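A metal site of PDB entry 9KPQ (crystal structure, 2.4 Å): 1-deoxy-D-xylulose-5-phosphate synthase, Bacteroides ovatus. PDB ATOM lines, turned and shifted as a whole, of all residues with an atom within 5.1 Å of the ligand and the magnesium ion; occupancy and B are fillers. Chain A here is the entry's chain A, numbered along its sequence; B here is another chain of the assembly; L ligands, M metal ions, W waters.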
ATOM      1  N   HIS A  44     -19.339   6.943 -23.741  1.00  0.00           N
ATOM      2  CA  HIS A  44     -17.890   6.879 -23.643  1.00  0.00           C
ATOM      3  C   HIS A  44     -17.235   6.800 -25.037  1.00  0.00           C
ATOM      4  O   HIS A  44     -17.075   5.718 -25.597  1.00  0.00           O
ATOM      5  CB  HIS A  44     -17.474   5.690 -22.753  1.00  0.00           C
ATOM      6  CG  HIS A  44     -17.761   5.906 -21.294  1.00  0.00           C
ATOM      7  ND1 HIS A  44     -18.942   5.524 -20.697  1.00  0.00           N
ATOM      8  CD2 HIS A  44     -17.035   6.517 -20.323  1.00  0.00           C
ATOM      9  CE1 HIS A  44     -18.925   5.860 -19.426  1.00  0.00           C
ATOM     10  NE2 HIS A  44     -17.771   6.462 -19.169  1.00  0.00           N
ATOM     11  N   PRO A  47     -12.879   5.703 -25.045  1.00  0.00           N
ATOM     12  CA  PRO A  47     -12.562   4.313 -24.691  1.00  0.00           C
ATOM     13  C   PRO A  47     -13.027   3.282 -25.734  1.00  0.00           C
ATOM     14  O   PRO A  47     -12.349   2.275 -25.907  1.00  0.00           O
ATOM     15  CB  PRO A  47     -13.322   4.105 -23.372  1.00  0.00           C
ATOM     16  CG  PRO A  47     -13.469   5.482 -22.794  1.00  0.00           C
ATOM     17  CD  PRO A  47     -13.659   6.375 -23.991  1.00  0.00           C
ATOM     18  N   VAL A  73     -14.502  -1.945 -15.434  1.00  0.00           N
ATOM     19  CA  VAL A  73     -15.469  -0.823 -15.532  1.00  0.00           C
ATOM     20  C   VAL A  73     -16.655  -1.109 -16.435  1.00  0.00           C
ATOM     21  O   VAL A  73     -17.776  -0.982 -16.041  1.00  0.00           O
ATOM     22  CB  VAL A  73     -14.877   0.570 -15.887  1.00  0.00           C
ATOM     23  CG1 VAL A  73     -15.932   1.621 -15.809  1.00  0.00           C
ATOM     24  CG2 VAL A  73     -13.721   0.929 -15.011  1.00  0.00           C
ATOM     25  N   HIS A  75     -17.301   0.428 -19.269  1.00  0.00           N
ATOM     26  CA  HIS A  75     -17.593   1.583 -20.016  1.00  0.00           C
ATOM     27  C   HIS A  75     -16.992   1.416 -21.457  1.00  0.00           C
ATOM     28  O   HIS A  75     -17.424   2.124 -22.314  1.00  0.00           O
ATOM     29  CB  HIS A  75     -16.933   2.778 -19.302  1.00  0.00           C
ATOM     30  CG  HIS A  75     -15.432   2.823 -19.455  1.00  0.00           C
ATOM     31  ND1 HIS A  75     -14.606   1.774 -19.127  1.00  0.00           N
ATOM     32  CD2 HIS A  75     -14.625   3.779 -19.922  1.00  0.00           C
ATOM     33  CE1 HIS A  75     -13.359   2.101 -19.363  1.00  0.00           C
ATOM     34  NE2 HIS A  75     -13.344   3.308 -19.864  1.00  0.00           N
ATOM     35  N   GLY A 116     -19.361  -1.291 -13.028  1.00  0.00           N
ATOM     36  CA  GLY A 116     -19.223   0.160 -13.246  1.00  0.00           C
ATOM     37  C   GLY A 116     -18.067   0.793 -12.467  1.00  0.00           C
ATOM     38  O   GLY A 116     -17.674   1.854 -12.876  1.00  0.00           O
ATOM     39  N   HIS A 117     -17.638   0.104 -11.433  1.00  0.00           N
ATOM     40  CA  HIS A 117     -16.545   0.660 -10.597  1.00  0.00           C
ATOM     41  C   HIS A 117     -15.208   0.161 -11.153  1.00  0.00           C
ATOM     42  O   HIS A 117     -15.193  -0.744 -11.978  1.00  0.00           O
ATOM     43  CB  HIS A 117     -16.793   0.426  -9.108  1.00  0.00           C
ATOM     44  CG  HIS A 117     -17.817   1.302  -8.494  1.00  0.00           C
ATOM     45  ND1 HIS A 117     -17.968   1.387  -7.138  1.00  0.00           N
ATOM     46  CD2 HIS A 117     -18.736   2.112  -9.016  1.00  0.00           C
ATOM     47  CE1 HIS A 117     -18.944   2.223  -6.858  1.00  0.00           C
ATOM     48  NE2 HIS A 117     -19.417   2.676  -7.985  1.00  0.00           N
ATOM     49  N   THR A 118     -14.114   0.733 -10.678  1.00  0.00           N
ATOM     50  CA  THR A 118     -12.812   0.440 -11.257  1.00  0.00           C
ATOM     51  C   THR A 118     -12.047  -0.675 -10.549  1.00  0.00           C
ATOM     52  O   THR A 118     -12.268  -0.942  -9.355  1.00  0.00           O
ATOM     53  CB  THR A 118     -11.940   1.669 -11.223  1.00  0.00           C
ATOM     54  OG1 THR A 118     -11.882   2.150  -9.870  1.00  0.00           O
ATOM     55  CG2 THR A 118     -12.510   2.738 -12.114  1.00  0.00           C
ATOM     56  N   GLY A 146      -7.968  -1.449 -18.063  1.00  0.00           N
ATOM     57  CA  GLY A 146      -7.293  -0.200 -18.418  1.00  0.00           C
ATOM     58  C   GLY A 146      -6.104   0.145 -17.529  1.00  0.00           C
ATOM     59  O   GLY A 146      -6.076  -0.231 -16.358  1.00  0.00           O
ATOM     60  N   ASP A 147      -5.144   0.876 -18.098  1.00  0.00           N
ATOM     61  CA  ASP A 147      -3.916   1.277 -17.411  1.00  0.00           C
ATOM     62  C   ASP A 147      -4.184   2.156 -16.188  1.00  0.00           C
ATOM     63  O   ASP A 147      -3.476   2.083 -15.194  1.00  0.00           O
ATOM     64  CB  ASP A 147      -2.963   2.019 -18.386  1.00  0.00           C
ATOM     65  CG  ASP A 147      -3.624   3.210 -19.096  1.00  0.00           C
ATOM     66  OD1 ASP A 147      -4.700   3.058 -19.719  1.00  0.00           O
ATOM     67  OD2 ASP A 147      -3.052   4.322 -19.039  1.00  0.00           O
ATOM     68  N   GLY A 148      -5.220   2.996 -16.262  1.00  0.00           N
ATOM     69  CA  GLY A 148      -5.603   3.755 -15.090  1.00  0.00           C
ATOM     70  C   GLY A 148      -6.123   2.909 -13.927  1.00  0.00           C
ATOM     71  O   GLY A 148      -5.792   3.149 -12.765  1.00  0.00           O
ATOM     72  N   SER A 149      -6.953   1.918 -14.264  1.00  0.00           N
ATOM     73  CA  SER A 149      -7.563   1.028 -13.260  1.00  0.00           C
ATOM     74  C   SER A 149      -6.491   0.230 -12.503  1.00  0.00           C
ATOM     75  O   SER A 149      -6.738  -0.306 -11.402  1.00  0.00           O
ATOM     76  CB  SER A 149      -8.550   0.048 -13.916  1.00  0.00           C
ATOM     77  OG  SER A 149      -9.816   0.652 -14.145  1.00  0.00           O
ATOM     78  N   ASN A 174      -4.963  -2.756 -21.315  1.00  0.00           N
ATOM     79  CA  ASN A 174      -5.243  -1.820 -22.408  1.00  0.00           C
ATOM     80  C   ASN A 174      -4.550  -0.489 -22.116  1.00  0.00           C
ATOM     81  O   ASN A 174      -5.132   0.417 -21.494  1.00  0.00           O
ATOM     82  CB  ASN A 174      -6.758  -1.632 -22.580  1.00  0.00           C
ATOM     83  CG  ASN A 174      -7.084  -0.635 -23.651  1.00  0.00           C
ATOM     84  OD1 ASN A 174      -6.221  -0.279 -24.449  1.00  0.00           O
ATOM     85  ND2 ASN A 174      -8.326  -0.178 -23.687  1.00  0.00           N
ATOM     86  N   ASN A 176      -3.445   2.903 -22.974  1.00  0.00           N
ATOM     87  CA  ASN A 176      -3.570   4.060 -23.870  1.00  0.00           C
ATOM     88  C   ASN A 176      -3.004   5.349 -23.261  1.00  0.00           C
ATOM     89  O   ASN A 176      -3.344   6.450 -23.699  1.00  0.00           O
ATOM     90  CB  ASN A 176      -5.039   4.287 -24.299  1.00  0.00           C
ATOM     91  CG  ASN A 176      -6.007   4.380 -23.110  1.00  0.00           C
ATOM     92  OD1 ASN A 176      -5.638   4.753 -21.987  1.00  0.00           O
ATOM     93  ND2 ASN A 176      -7.283   4.058 -23.374  1.00  0.00           N
ATOM     94  N   GLN A 177      -2.160   5.199 -22.232  1.00  0.00           N
ATOM     95  CA  GLN A 177      -1.481   6.326 -21.558  1.00  0.00           C
ATOM     96  C   GLN A 177      -2.427   7.415 -21.037  1.00  0.00           C
ATOM     97  O   GLN A 177      -2.080   8.586 -21.012  1.00  0.00           O
ATOM     98  CB  GLN A 177      -0.452   6.959 -22.501  1.00  0.00           C
ATOM     99  CG  GLN A 177       0.595   5.966 -23.033  1.00  0.00           C
ATOM    100  CD  GLN A 177       0.146   5.273 -24.323  1.00  0.00           C
ATOM    101  OE1 GLN A 177      -0.102   5.928 -25.342  1.00  0.00           O
ATOM    102  NE2 GLN A 177       0.044   3.952 -24.281  1.00  0.00           N
ATOM    103  N   MET A 178      -3.602   7.018 -20.581  1.00  0.00           N
ATOM    104  CA  MET A 178      -4.627   7.970 -20.127  1.00  0.00           C
ATOM    105  C   MET A 178      -5.515   7.261 -19.126  1.00  0.00           C
ATOM    106  O   MET A 178      -5.839   6.093 -19.292  1.00  0.00           O
ATOM    107  CB  MET A 178      -5.480   8.442 -21.297  1.00  0.00           C
ATOM    108  CG  MET A 178      -5.068   9.712 -22.029  1.00  0.00           C
ATOM    109  SD  MET A 178      -4.338  10.988 -21.006  1.00  0.00           S
ATOM    110  CE  MET A 178      -5.698  12.136 -20.789  1.00  0.00           C
ATOM    111  N   SER A 179      -5.903   7.959 -18.063  1.00  0.00           N
ATOM    112  CA  SER A 179      -7.008   7.476 -17.249  1.00  0.00           C
ATOM    113  C   SER A 179      -8.232   8.206 -17.782  1.00  0.00           C
ATOM    114  O   SER A 179      -8.557   8.055 -18.961  1.00  0.00           O
ATOM    115  CB  SER A 179      -6.776   7.743 -15.752  1.00  0.00           C
ATOM    116  OG  SER A 179      -7.775   7.163 -14.954  1.00  0.00           O
ATOM    117  N   ILE A 180      -8.881   9.010 -16.948  1.00  0.00           N
ATOM    118  CA  ILE A 180      -9.747  10.066 -17.470  1.00  0.00           C
ATOM    119  C   ILE A 180      -8.939  11.338 -17.823  1.00  0.00           C
ATOM    120  O   ILE A 180      -8.850  11.737 -18.994  1.00  0.00           O
ATOM    121  CB  ILE A 180     -10.825  10.492 -16.458  1.00  0.00           C
ATOM    122  CG1 ILE A 180     -11.761   9.329 -16.121  1.00  0.00           C
ATOM    123  CG2 ILE A 180     -11.578  11.715 -16.976  1.00  0.00           C
ATOM    124  CD1 ILE A 180     -12.955   9.736 -15.260  1.00  0.00           C
ATOM    125  N   ASN A 183      -2.564   9.816 -16.143  1.00  0.00           N
ATOM    126  CA  ASN A 183      -2.267   8.886 -15.063  1.00  0.00           C
ATOM    127  C   ASN A 183      -1.302   9.481 -14.019  1.00  0.00           C
ATOM    128  O   ASN A 183      -0.609  10.462 -14.290  1.00  0.00           O
ATOM    129  CB  ASN A 183      -1.681   7.597 -15.654  1.00  0.00           C
ATOM    130  CG  ASN A 183      -2.680   6.853 -16.512  1.00  0.00           C
ATOM    131  OD1 ASN A 183      -3.798   6.587 -16.085  1.00  0.00           O
ATOM    132  ND2 ASN A 183      -2.281   6.503 -17.730  1.00  0.00           N
ATOM    133  N   LYS A 247      -6.160   6.150 -27.700  1.00  0.00           N
ATOM    134  CA  LYS A 247      -7.470   6.519 -27.188  1.00  0.00           C
ATOM    135  C   LYS A 247      -8.245   7.384 -28.178  1.00  0.00           C
ATOM    136  O   LYS A 247      -7.813   8.497 -28.515  1.00  0.00           O
ATOM    137  CB  LYS A 247      -7.343   7.242 -25.847  1.00  0.00           C
ATOM    138  CG  LYS A 247      -8.675   7.529 -25.171  1.00  0.00           C
ATOM    139  CD  LYS A 247      -8.576   7.268 -23.666  1.00  0.00           C
ATOM    140  CE  LYS A 247      -9.952   7.211 -23.034  1.00  0.00           C
ATOM    141  NZ  LYS A 247      -9.943   7.564 -21.608  1.00  0.00           N
ATOM    142  N   HIS A 262     -13.278  11.366 -23.258  1.00  0.00           N
ATOM    143  CA  HIS A 262     -13.516  10.179 -22.468  1.00  0.00           C
ATOM    144  C   HIS A 262     -15.021   9.920 -22.326  1.00  0.00           C
ATOM    145  O   HIS A 262     -15.476   8.778 -22.420  1.00  0.00           O
ATOM    146  CB  HIS A 262     -12.852  10.303 -21.080  1.00  0.00           C
ATOM    147  CG  HIS A 262     -13.191   9.175 -20.152  1.00  0.00           C
ATOM    148  ND1 HIS A 262     -12.444   8.018 -20.103  1.00  0.00           N
ATOM    149  CD2 HIS A 262     -14.200   9.020 -19.270  1.00  0.00           C
ATOM    150  CE1 HIS A 262     -12.975   7.208 -19.205  1.00  0.00           C
ATOM    151  NE2 HIS A 262     -14.036   7.785 -18.690  1.00  0.00           N
ATOM    152  N   SER A 306      -9.180  11.443  -6.523  1.00  0.00           N
ATOM    153  CA  SER A 306      -8.823  10.056  -6.796  1.00  0.00           C
ATOM    154  C   SER A 306      -9.342   9.977  -8.241  1.00  0.00           C
ATOM    155  O   SER A 306     -10.513   9.602  -8.484  1.00  0.00           O
ATOM    156  CB  SER A 306      -9.500   9.085  -5.791  1.00  0.00           C
ATOM    157  OG  SER A 306     -10.805   9.523  -5.395  1.00  0.00           O
ATOM    158  N   GLY A 307      -8.488  10.360  -9.194  1.00  0.00           N
ATOM    159  CA  GLY A 307      -8.672  10.114 -10.614  1.00  0.00           C
ATOM    160  C   GLY A 307      -9.883  10.790 -11.269  1.00  0.00           C
ATOM    161  O   GLY A 307     -10.201  10.509 -12.417  1.00  0.00           O
ATOM    162  N   THR A 308     -10.583  11.642 -10.534  1.00  0.00           N
ATOM    163  CA  THR A 308     -11.771  12.306 -11.069  1.00  0.00           C
ATOM    164  C   THR A 308     -11.698  13.810 -10.641  1.00  0.00           C
ATOM    165  O   THR A 308     -12.482  14.248  -9.797  1.00  0.00           O
ATOM    166  CB  THR A 308     -13.091  11.647 -10.494  1.00  0.00           C
ATOM    167  OG1 THR A 308     -13.249  11.960  -9.094  1.00  0.00           O
ATOM    168  CG2 THR A 308     -13.059  10.126 -10.640  1.00  0.00           C
ATOM    169  N   ILE A 331      -6.704   6.152  -9.160  1.00  0.00           N
ATOM    170  CA  ILE A 331      -8.033   5.720  -8.764  1.00  0.00           C
ATOM    171  C   ILE A 331      -7.940   4.922  -7.470  1.00  0.00           C
ATOM    172  O   ILE A 331      -8.245   3.722  -7.413  1.00  0.00           O
ATOM    173  CB  ILE A 331      -8.693   4.932  -9.886  1.00  0.00           C
ATOM    174  CG1 ILE A 331      -8.385   5.588 -11.229  1.00  0.00           C
ATOM    175  CG2 ILE A 331     -10.176   4.919  -9.684  1.00  0.00           C
ATOM    176  CD1 ILE A 331      -8.605   4.659 -12.415  1.00  0.00           C
ATOM    177  N   GLU A 333      -9.184   5.553  -3.895  1.00  0.00           N
ATOM    178  CA  GLU A 333     -10.019   6.160  -2.863  1.00  0.00           C
ATOM    179  C   GLU A 333      -9.569   5.842  -1.431  1.00  0.00           C
ATOM    180  O   GLU A 333      -9.656   6.674  -0.529  1.00  0.00           O
ATOM    181  CB  GLU A 333     -11.464   5.709  -3.029  1.00  0.00           C
ATOM    182  CG  GLU A 333     -12.174   6.289  -4.241  1.00  0.00           C
ATOM    183  CD  GLU A 333     -11.937   5.501  -5.516  1.00  0.00           C
ATOM    184  OE1 GLU A 333     -11.041   4.612  -5.513  1.00  0.00           O
ATOM    185  OE2 GLU A 333     -12.641   5.765  -6.524  1.00  0.00           O
ATOM    186  N   PHE A 358     -18.418   6.422  -5.305  1.00  0.00           N
ATOM    187  CA  PHE A 358     -17.030   5.924  -5.265  1.00  0.00           C
ATOM    188  C   PHE A 358     -16.446   5.899  -3.857  1.00  0.00           C
ATOM    189  O   PHE A 358     -15.617   5.031  -3.543  1.00  0.00           O
ATOM    190  CB  PHE A 358     -16.137   6.740  -6.207  1.00  0.00           C
ATOM    191  CG  PHE A 358     -16.517   6.620  -7.656  1.00  0.00           C
ATOM    192  CD1 PHE A 358     -17.187   5.493  -8.113  1.00  0.00           C
ATOM    193  CD2 PHE A 358     -16.254   7.641  -8.553  1.00  0.00           C
ATOM    194  CE1 PHE A 358     -17.556   5.373  -9.445  1.00  0.00           C
ATOM    195  CE2 PHE A 358     -16.613   7.539  -9.893  1.00  0.00           C
ATOM    196  CZ  PHE A 358     -17.277   6.412 -10.342  1.00  0.00           C
ATOM    197  N   ARG A 361     -15.702   2.805  -1.341  1.00  0.00           N
ATOM    198  CA  ARG A 361     -14.505   1.965  -1.237  1.00  0.00           C
ATOM    199  C   ARG A 361     -13.751   2.151   0.084  1.00  0.00           C
ATOM    200  O   ARG A 361     -12.979   1.268   0.478  1.00  0.00           O
ATOM    201  CB  ARG A 361     -13.516   2.258  -2.391  1.00  0.00           C
ATOM    202  CG  ARG A 361     -13.893   1.729  -3.769  1.00  0.00           C
ATOM    203  CD  ARG A 361     -13.653   0.243  -3.882  1.00  0.00           C
ATOM    204  NE  ARG A 361     -14.273  -0.325  -5.081  1.00  0.00           N
ATOM    205  CZ  ARG A 361     -13.677  -0.396  -6.268  1.00  0.00           C
ATOM    206  NH1 ARG A 361     -12.423   0.007  -6.448  1.00  0.00           N
ATOM    207  NH2 ARG A 361     -14.344  -0.890  -7.296  1.00  0.00           N
ATOM    208  N   HIS A 394     -23.636   3.142 -10.471  1.00  0.00           N
ATOM    209  CA  HIS A 394     -23.283   4.492 -10.064  1.00  0.00           C
ATOM    210  C   HIS A 394     -24.340   5.184  -9.203  1.00  0.00           C
ATOM    211  O   HIS A 394     -24.395   6.404  -9.155  1.00  0.00           O
ATOM    212  CB  HIS A 394     -22.969   5.351 -11.287  1.00  0.00           C
ATOM    213  CG  HIS A 394     -21.735   4.923 -12.003  1.00  0.00           C
ATOM    214  ND1 HIS A 394     -21.703   3.839 -12.855  1.00  0.00           N
ATOM    215  CD2 HIS A 394     -20.465   5.386 -11.958  1.00  0.00           C
ATOM    216  CE1 HIS A 394     -20.481   3.680 -13.325  1.00  0.00           C
ATOM    217  NE2 HIS A 394     -19.706   4.598 -12.785  1.00  0.00           N
ATOM    218  N   ASP B 364     -17.591  -1.718  -0.632  1.00  0.00           N
ATOM    219  CA  ASP B 364     -17.904  -1.560  -2.054  1.00  0.00           C
ATOM    220  C   ASP B 364     -17.875  -2.915  -2.780  1.00  0.00           C
ATOM    221  O   ASP B 364     -18.584  -3.136  -3.775  1.00  0.00           O
ATOM    222  CB  ASP B 364     -16.923  -0.580  -2.736  1.00  0.00           C
ATOM    223  CG  ASP B 364     -17.428  -0.093  -4.088  1.00  0.00           C
ATOM    224  OD1 ASP B 364     -18.569   0.376  -4.162  1.00  0.00           O
ATOM    225  OD2 ASP B 364     -16.684  -0.176  -5.088  1.00  0.00           O
HETATM  226  N1  LIG L   1     -13.452   4.927  -8.977  1.00  0.00           N
HETATM  227  C1  LIG L   1     -14.281   3.872  -9.141  1.00  0.00           C
HETATM  228  C2  LIG L   1     -14.363   2.876  -8.042  1.00  0.00           C
HETATM  229  N2  LIG L   1     -15.054   3.662 -10.225  1.00  0.00           N
HETATM  230  C3  LIG L   1     -14.998   4.530 -11.219  1.00  0.00           C
HETATM  231  N3  LIG L   1     -15.783   4.291 -12.294  1.00  0.00           N
HETATM  232  C4  LIG L   1     -14.130   5.690 -11.170  1.00  0.00           C
HETATM  233  C5  LIG L   1     -13.406   5.805  -9.988  1.00  0.00           C
HETATM  234  C6  LIG L   1     -14.051   6.750 -12.241  1.00  0.00           C
HETATM  235  N4  LIG L   1     -13.820   6.246 -13.622  1.00  0.00           N
HETATM  236  C7  LIG L   1     -14.796   5.848 -14.432  1.00  0.00           C
HETATM  237  S1  LIG L   1     -14.227   5.393 -15.951  1.00  0.00           S
HETATM  238  C8  LIG L   1     -12.602   5.784 -15.509  1.00  0.00           C
HETATM  239  C9  LIG L   1     -12.559   6.252 -14.207  1.00  0.00           C
HETATM  240  C10 LIG L   1     -11.366   6.717 -13.432  1.00  0.00           C
HETATM  241  C11 LIG L   1     -11.467   5.618 -16.487  1.00  0.00           C
HETATM  242  C12 LIG L   1     -10.549   4.455 -16.154  1.00  0.00           C
HETATM  243  O1  LIG L   1      -9.308   4.632 -16.884  1.00  0.00           O
HETATM  244  P1  LIG L   1      -8.628   3.504 -17.768  1.00  0.00           P
HETATM  245  O2  LIG L   1      -7.173   3.711 -17.997  1.00  0.00           O
HETATM  246  O3  LIG L   1      -9.016   2.174 -17.103  1.00  0.00           O
HETATM  247  O4  LIG L   1      -9.444   3.645 -19.166  1.00  0.00           O
HETATM  248  P2  LIG L   1      -9.557   4.634 -20.407  1.00  0.00           P
HETATM  249  O5  LIG L   1     -10.508   5.742 -20.119  1.00  0.00           O
HETATM  250  O6  LIG L   1     -10.055   3.741 -21.636  1.00  0.00           O
HETATM  251  O7  LIG L   1      -8.099   5.083 -20.649  1.00  0.00           O
HETATM  252 MG    MG M   1      -6.395   3.943 -19.877  1.00  0.00          MG
HETATM  253  O   HOH W   1      -7.066   2.176 -20.848  1.00  0.00           O
HETATM  254  O   HOH W   2     -10.602  -0.223 -17.251  1.00  0.00           O
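Water W1 lies within hydrogen-bond range of the backbone carbonyl oxygen (O) of Asn 174 (2.7 Å), the side-chain amide nitrogen (ND2) of Asn 176 (3.2 Å) and an oxygen (O4) of the ligand (3.3 Å). Water W2 lies within hydrogen-bond range of an oxygen (O3) of the ligand, the backbone NH (N) of Gly 146 and the side-chain hydroxyl (OG) of Ser 149.
The backbone carbonyl oxygen of Ser 179 sits close to an oxygen (O5) of the ligand (3.2 Å). Merely in contact with the ligand: Phe 358, Gly 146, Ile 331, His 117, Ile 180, Pro 47, His 75, Arg 361, Thr 308 and His 394. 21 residues have an atom within 4 Å of the ligand: Pro 47, His 75, Gly 116, His 117, Thr 118, Gly 146, Asp 147, Gly 148, Ser 149, Asn 176, Met 178, Ser 179, Ile 180, Lys 247, His 262, Thr 308, Ile 331, Glu 333, Phe 358, Arg 361 and His 394.
The backbone carbonyl oxygen of Asn 174 lies within hydrogen-bond range of the backbone NH of Asp 147 (3.4 Å). The side-chain carboxylate (OD2) of Asp 147 sits at hydrogen-bond distance from the side-chain amide nitrogen (ND2) of Asn 183, at 2.7 Å. The side-chain carboxylate (OD2) of Asp 147 lies within hydrogen-bond range of the backbone NH (N) of Gln 177 (3.4 Å). N of Met 178 sits close to ND2 of Asn 183 (3.2 Å). NZ of Lys 247 is in hydrogen-bond range of ND1 of His 262, at 3.0 Å. The side-chain amino group (NZ) of Lys 247 lies within hydrogen-bond range of the backbone carbonyl oxygen (O) of Ser 179 (3.0 Å). A ring nitrogen (ND1) of His 117 is in hydrogen-bond range of the side-chain carboxylate (OD2) of Asp 364 of chain B (2.9 Å). The side-chain carboxylate (OD2) of Asp 364 of chain B lies within salt-bridge range of the guanidinium group (NE) of Arg 361, 2.4 Å away.
The magnesium ion is bound by OD1 of Asp 147 (1.9 Å). O2 of the ligand binds the magnesium ion, at 2.0 Å. The magnesium ion is bound by water W1. O7 of the ligand is bound to the magnesium ion. O of Met 178 binds the magnesium ion. The magnesium ion is bound by the side-chain amide oxygen (OD1) of Asn 176. The magnesium ion has six donor atoms within binding distance.
The backbone NH (N) of Asp 147 sits close to an oxygen (O2) of the ligand, at 3.5 Å. The side-chain amino group (NZ) of Lys 247 lies within salt-bridge range of an oxygen (O5) of the ligand (2.4 Å). N of Gly 148 lies close to O2 of the ligand (2.7 Å). A nitrogen (N1) of the ligand is in hydrogen-bond range of the side-chain carboxylate of Glu 333 (2.7 Å). O5 of the ligand sits at hydrogen-bond distance from ND1 of His 262, 3.0 Å away. N of Thr 118 is in hydrogen-bond range of N2 of the ligand, 3.1 Å away. A nitrogen (N1) of the ligand sits close to the side-chain hydroxyl (OG1) of Thr 118, 3.3 Å away. The backbone carbonyl oxygen of Gly 116 is in hydrogen-bond range of a nitrogen (N3) of the ligand (3.1 Å). O3 of the ligand lies within hydrogen-bond range of OG of Ser 149 (3.4 Å).
Gly 148 touches the magnesium ion. Four residues have an atom within 4 Å of the magnesium ion: Asp 147, Gly 148, Asn 176 and Met 178. Along chain A the residues within 4 Å of the magnesium ion span positions 147 to 178.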
